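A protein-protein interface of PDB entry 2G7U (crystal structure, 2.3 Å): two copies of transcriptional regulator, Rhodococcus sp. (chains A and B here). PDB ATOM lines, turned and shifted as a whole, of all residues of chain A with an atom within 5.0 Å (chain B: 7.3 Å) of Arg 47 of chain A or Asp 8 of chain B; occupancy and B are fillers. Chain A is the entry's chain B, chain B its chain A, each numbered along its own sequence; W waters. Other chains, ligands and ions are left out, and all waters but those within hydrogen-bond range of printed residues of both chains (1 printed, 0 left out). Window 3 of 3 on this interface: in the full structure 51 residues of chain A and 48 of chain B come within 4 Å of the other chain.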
ATOM      1  N   LEU A  32      -4.475   8.830 -32.329  1.00  0.00           N
ATOM      2  CA  LEU A  32      -3.852  10.134 -32.080  1.00  0.00           C
ATOM      3  C   LEU A  32      -3.167  10.674 -33.340  1.00  0.00           C
ATOM      4  O   LEU A  32      -3.420  11.803 -33.754  1.00  0.00           O
ATOM      5  CB  LEU A  32      -2.821  10.028 -30.955  1.00  0.00           C
ATOM      6  CG  LEU A  32      -2.106  11.341 -30.554  1.00  0.00           C
ATOM      7  CD1 LEU A  32      -2.815  11.923 -29.403  1.00  0.00           C
ATOM      8  CD2 LEU A  32      -0.684  11.053 -30.130  1.00  0.00           C
ATOM      9  N   ARG A  43       2.332  15.645 -32.220  1.00  0.00           N
ATOM     10  CA  ARG A  43       1.702  14.647 -31.364  1.00  0.00           C
ATOM     11  C   ARG A  43       1.692  15.018 -29.853  1.00  0.00           C
ATOM     12  O   ARG A  43       0.686  14.808 -29.188  1.00  0.00           O
ATOM     13  CB  ARG A  43       2.280  13.254 -31.642  1.00  0.00           C
ATOM     14  CG  ARG A  43       2.551  12.396 -30.384  1.00  0.00           C
ATOM     15  CD  ARG A  43       2.906  10.940 -30.748  1.00  0.00           C
ATOM     16  NE  ARG A  43       2.206  10.009 -29.860  1.00  0.00           N
ATOM     17  CZ  ARG A  43       1.429   9.012 -30.277  1.00  0.00           C
ATOM     18  NH1 ARG A  43       1.259   8.779 -31.582  1.00  0.00           N
ATOM     19  NH2 ARG A  43       0.831   8.234 -29.384  1.00  0.00           N
ATOM     20  N   PRO A  44       2.808  15.559 -29.300  1.00  0.00           N
ATOM     21  CA  PRO A  44       2.704  16.030 -27.905  1.00  0.00           C
ATOM     22  C   PRO A  44       1.619  17.099 -27.646  1.00  0.00           C
ATOM     23  O   PRO A  44       0.991  17.097 -26.570  1.00  0.00           O
ATOM     24  CB  PRO A  44       4.106  16.583 -27.620  1.00  0.00           C
ATOM     25  CG  PRO A  44       4.975  15.837 -28.547  1.00  0.00           C
ATOM     26  CD  PRO A  44       4.184  15.716 -29.805  1.00  0.00           C
ATOM     27  N   ALA A  45       1.395  17.987 -28.616  1.00  0.00           N
ATOM     28  CA  ALA A  45       0.402  19.037 -28.479  1.00  0.00           C
ATOM     29  C   ALA A  45      -0.961  18.409 -28.470  1.00  0.00           C
ATOM     30  O   ALA A  45      -1.794  18.723 -27.610  1.00  0.00           O
ATOM     31  CB  ALA A  45       0.500  20.050 -29.619  1.00  0.00           C
ATOM     32  N   VAL A  46      -1.171  17.510 -29.432  1.00  0.00           N
ATOM     33  CA  VAL A  46      -2.458  16.850 -29.610  1.00  0.00           C
ATOM     34  C   VAL A  46      -2.786  15.954 -28.424  1.00  0.00           C
ATOM     35  O   VAL A  46      -3.918  15.987 -27.938  1.00  0.00           O
ATOM     36  CB  VAL A  46      -2.548  16.121 -30.980  1.00  0.00           C
ATOM     37  CG1 VAL A  46      -3.754  15.219 -31.048  1.00  0.00           C
ATOM     38  CG2 VAL A  46      -2.645  17.150 -32.075  1.00  0.00           C
ATOM     39  N   ARG A  47      -1.791  15.197 -27.946  1.00  0.00           N
ATOM     40  CA  ARG A  47      -1.963  14.368 -26.748  1.00  0.00           C
ATOM     41  C   ARG A  47      -2.403  15.183 -25.519  1.00  0.00           C
ATOM     42  O   ARG A  47      -3.281  14.751 -24.757  1.00  0.00           O
ATOM     43  CB  ARG A  47      -0.691  13.588 -26.411  1.00  0.00           C
ATOM     44  CG  ARG A  47      -0.912  12.481 -25.380  1.00  0.00           C
ATOM     45  CD  ARG A  47       0.396  11.954 -24.819  1.00  0.00           C
ATOM     46  NE  ARG A  47       0.561  12.268 -23.397  1.00  0.00           N
ATOM     47  CZ  ARG A  47       0.325  11.416 -22.395  1.00  0.00           C
ATOM     48  NH1 ARG A  47      -0.097  10.173 -22.633  1.00  0.00           N
ATOM     49  NH2 ARG A  47       0.513  11.809 -21.142  1.00  0.00           N
ATOM     50  N   ARG A  48      -1.778  16.345 -25.321  1.00  0.00           N
ATOM     51  CA  ARG A  48      -2.120  17.191 -24.185  1.00  0.00           C
ATOM     52  C   ARG A  48      -3.541  17.768 -24.339  1.00  0.00           C
ATOM     53  O   ARG A  48      -4.299  17.816 -23.376  1.00  0.00           O
ATOM     54  CB  ARG A  48      -1.076  18.298 -24.022  1.00  0.00           C
ATOM     55  CG  ARG A  48      -1.115  19.014 -22.677  1.00  0.00           C
ATOM     56  CD  ARG A  48       0.047  20.008 -22.579  1.00  0.00           C
ATOM     57  NE  ARG A  48       0.101  20.648 -21.268  1.00  0.00           N
ATOM     58  CZ  ARG A  48       0.327  21.947 -21.056  1.00  0.00           C
ATOM     59  NH1 ARG A  48       0.546  22.785 -22.066  1.00  0.00           N
ATOM     60  NH2 ARG A  48       0.343  22.402 -19.818  1.00  0.00           N
ATOM     61  N   ILE A  49      -3.884  18.190 -25.554  1.00  0.00           N
ATOM     62  CA  ILE A  49      -5.226  18.686 -25.848  1.00  0.00           C
ATOM     63  C   ILE A  49      -6.295  17.598 -25.653  1.00  0.00           C
ATOM     64  O   ILE A  49      -7.358  17.845 -25.046  1.00  0.00           O
ATOM     65  CB  ILE A  49      -5.316  19.288 -27.256  1.00  0.00           C
ATOM     66  CG1 ILE A  49      -4.429  20.538 -27.323  1.00  0.00           C
ATOM     67  CG2 ILE A  49      -6.759  19.697 -27.548  1.00  0.00           C
ATOM     68  CD1 ILE A  49      -4.019  20.955 -28.713  1.00  0.00           C
ATOM     69  N   LEU A  50      -6.004  16.396 -26.139  1.00  0.00           N
ATOM     70  CA  LEU A  50      -6.933  15.273 -26.012  1.00  0.00           C
ATOM     71  C   LEU A  50      -7.211  14.932 -24.554  1.00  0.00           C
ATOM     72  O   LEU A  50      -8.377  14.725 -24.165  1.00  0.00           O
ATOM     73  CB  LEU A  50      -6.392  14.042 -26.748  1.00  0.00           C
ATOM     74  CG  LEU A  50      -6.647  14.105 -28.248  1.00  0.00           C
ATOM     75  CD1 LEU A  50      -5.903  12.990 -29.016  1.00  0.00           C
ATOM     76  CD2 LEU A  50      -8.174  14.071 -28.498  1.00  0.00           C
ATOM     77  N   LEU A  51      -6.146  14.870 -23.754  1.00  0.00           N
ATOM     78  CA  LEU A  51      -6.274  14.580 -22.330  1.00  0.00           C
ATOM     79  C   LEU A  51      -7.091  15.653 -21.583  1.00  0.00           C
ATOM     80  O   LEU A  51      -7.827  15.341 -20.636  1.00  0.00           O
ATOM     81  CB  LEU A  51      -4.895  14.368 -21.682  1.00  0.00           C
ATOM     82  CG  LEU A  51      -4.155  13.046 -21.960  1.00  0.00           C
ATOM     83  CD1 LEU A  51      -2.750  13.068 -21.367  1.00  0.00           C
ATOM     84  CD2 LEU A  51      -4.924  11.833 -21.441  1.00  0.00           C
ATOM     85  N   THR A  52      -6.960  16.906 -22.018  1.00  0.00           N
ATOM     86  CA  THR A  52      -7.721  18.016 -21.441  1.00  0.00           C
ATOM     87  C   THR A  52      -9.186  17.904 -21.843  1.00  0.00           C
ATOM     88  O   THR A  52     -10.101  18.037 -20.996  1.00  0.00           O
ATOM     89  CB  THR A  52      -7.148  19.388 -21.866  1.00  0.00           C
ATOM     90  OG1 THR A  52      -5.796  19.477 -21.425  1.00  0.00           O
ATOM     91  CG2 THR A  52      -7.945  20.537 -21.229  1.00  0.00           C
ATOM     92  N   ASP B   6       5.751  15.963 -18.635  1.00  0.00           N
ATOM     93  CA  ASP B   6       4.608  16.490 -19.448  1.00  0.00           C
ATOM     94  C   ASP B   6       3.333  16.735 -18.620  1.00  0.00           C
ATOM     95  O   ASP B   6       2.761  15.804 -18.032  1.00  0.00           O
ATOM     96  CB  ASP B   6       4.341  15.575 -20.656  1.00  0.00           C
ATOM     97  CG  ASP B   6       5.375  15.758 -21.753  1.00  0.00           C
ATOM     98  OD1 ASP B   6       5.225  15.197 -22.867  1.00  0.00           O
ATOM     99  OD2 ASP B   6       6.348  16.492 -21.487  1.00  0.00           O
ATOM    100  N   ARG B   7       2.911  17.998 -18.546  1.00  0.00           N
ATOM    101  CA  ARG B   7       1.602  18.313 -17.995  1.00  0.00           C
ATOM    102  C   ARG B   7       0.606  17.774 -19.010  1.00  0.00           C
ATOM    103  O   ARG B   7       0.820  17.852 -20.233  1.00  0.00           O
ATOM    104  CB  ARG B   7       1.428  19.817 -17.766  1.00  0.00           C
ATOM    105  CG  ARG B   7       0.117  20.280 -17.109  1.00  0.00           C
ATOM    106  CD  ARG B   7      -0.148  19.645 -15.754  1.00  0.00           C
ATOM    107  NE  ARG B   7      -1.067  18.518 -15.936  1.00  0.00           N
ATOM    108  CZ  ARG B   7      -1.343  17.585 -15.029  1.00  0.00           C
ATOM    109  NH1 ARG B   7      -0.776  17.620 -13.831  1.00  0.00           N
ATOM    110  NH2 ARG B   7      -2.193  16.607 -15.326  1.00  0.00           N
ATOM    111  N   ASP B   8      -0.449  17.172 -18.479  1.00  0.00           N
ATOM    112  CA  ASP B   8      -1.499  16.584 -19.278  1.00  0.00           C
ATOM    113  C   ASP B   8      -2.745  17.459 -19.214  1.00  0.00           C
ATOM    114  O   ASP B   8      -3.830  17.028 -19.616  1.00  0.00           O
ATOM    115  CB  ASP B   8      -1.791  15.168 -18.772  1.00  0.00           C
ATOM    116  CG  ASP B   8      -0.542  14.293 -18.740  1.00  0.00           C
ATOM    117  OD1 ASP B   8       0.434  14.626 -19.442  1.00  0.00           O
ATOM    118  OD2 ASP B   8      -0.534  13.277 -18.014  1.00  0.00           O
ATOM    119  N   TYR B   9      -2.587  18.692 -18.724  1.00  0.00           N
ATOM    120  CA  TYR B   9      -3.742  19.561 -18.556  1.00  0.00           C
ATOM    121  C   TYR B   9      -3.547  21.018 -18.978  1.00  0.00           C
ATOM    122  O   TYR B   9      -2.688  21.710 -18.454  1.00  0.00           O
ATOM    123  CB  TYR B   9      -4.278  19.473 -17.121  1.00  0.00           C
ATOM    124  CG  TYR B   9      -5.728  19.892 -17.050  1.00  0.00           C
ATOM    125  CD1 TYR B   9      -6.739  19.050 -17.534  1.00  0.00           C
ATOM    126  CD2 TYR B   9      -6.089  21.143 -16.537  1.00  0.00           C
ATOM    127  CE1 TYR B   9      -8.088  19.445 -17.497  1.00  0.00           C
ATOM    128  CE2 TYR B   9      -7.435  21.556 -16.496  1.00  0.00           C
ATOM    129  CZ  TYR B   9      -8.425  20.699 -16.978  1.00  0.00           C
ATOM    130  OH  TYR B   9      -9.742  21.088 -16.937  1.00  0.00           O
ATOM    131  N   ILE B  10      -4.375  21.485 -19.905  1.00  0.00           N
ATOM    132  CA  ILE B  10      -4.325  22.873 -20.354  1.00  0.00           C
ATOM    133  C   ILE B  10      -5.513  23.650 -19.789  1.00  0.00           C
ATOM    134  O   ILE B  10      -6.640  23.573 -20.311  1.00  0.00           O
ATOM    135  CB  ILE B  10      -4.243  22.968 -21.899  1.00  0.00           C
ATOM    136  CG1 ILE B  10      -3.032  22.163 -22.423  1.00  0.00           C
ATOM    137  CG2 ILE B  10      -4.198  24.444 -22.382  1.00  0.00           C
ATOM    138  CD1 ILE B  10      -3.161  21.726 -23.884  1.00  0.00           C
HETATM  139  O   HOH W   1       2.794  12.927 -19.816  1.00  0.00           O
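Among the printed residues, pairs that only touch across the chains: Leu 51 of chain A with Asp 8 of chain B (3.5 Å), Thr 52 of chain A with Tyr 9 of chain B (3.5 Å), Arg 48 of chain A with Ile 10 of chain B (3.6 Å), Thr 52 of chain A with Asp 8 of chain B (3.6 Å), Ile 49 of chain A with Ile 10 of chain B (3.9 Å) and Arg 48 of chain A with Asp 8 of chain B (3.9 Å).
Of the 5 printed residues of chain B, 4 touch a printed residue of chain A. Of the 11 printed residues of chain A, 5 touch a printed residue of chain B. Hydrophobic or aromatic side chains of chain A within 4 Å of the printed part of chain B: Ile 49 and Leu 51. Among the printed residues, 10 pairs touch across the chains. Among the printed residues, Asp or Glu carboxylates within 4 Å of a Lys or Arg side-chain nitrogen of the other chain: Arg 47 of chain A with Asp 8 of chain B.
Water W1 lies within hydrogen-bond range of NH2 of Arg 47 of chain A (2.9 Å), OD1 of Asp 8 of chain B (2.9 Å) and O of Asp 6 of chain B (3.4 Å).
Of chain B, only Asp 8 (3.3 Å) comes within 4 Å of Arg 47 of chain A. Printed residues of chain A within 4 Å of Ile 10 of chain B: Arg 48 (3.6 Å), Ile 49 (3.9 Å) and Thr 52 (2.9 Å). Printed residues of chain B within 4 Å of Ile 49 of chain A: Ile 10 (3.9 Å). Of the printed residues of chain A, Arg 7 of chain B touches Arg 48. Printed residues of chain B within 4 Å of Thr 52 of chain A: Asp 8, Tyr 9 and Ile 10. Leu 50 of chain A touches none of the printed residues of chain B. Asp 6 of chain B touches none of the printed residues of chain A. The nearest printed residue of chain A that does not touch Asp 8 of chain B is Ile 49 of chain A (6.1 Å).
No position is printed for both chains. Of the 10 pairs that touch across the chains among the printed residues, none has its exchanged pair printed and touching as well.
The backbone carbonyl oxygen of Arg 7 of chain B lies within hydrogen-bond range of the guanidinium group of Arg 48 of chain A, 3.1 Å away. The side-chain carboxylate of Asp 8 of chain B is in salt-bridge range of the guanidinium group of Arg 47 of chain A (3.3 Å). The guanidinium group (NH2) of Arg 48 of chain A lies within hydrogen-bond range of the backbone carbonyl oxygen (O) of Tyr 9 of chain B (3.4 Å). N of Ile 10 of chain B lies within hydrogen-bond range of OG1 of Thr 52 of chain A (2.9 Å).
The backbone carbonyl oxygen of Arg 48 of chain A is in hydrogen-bond range of the side-chain hydroxyl of Thr 52 of chain A, at 3.0 Å.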
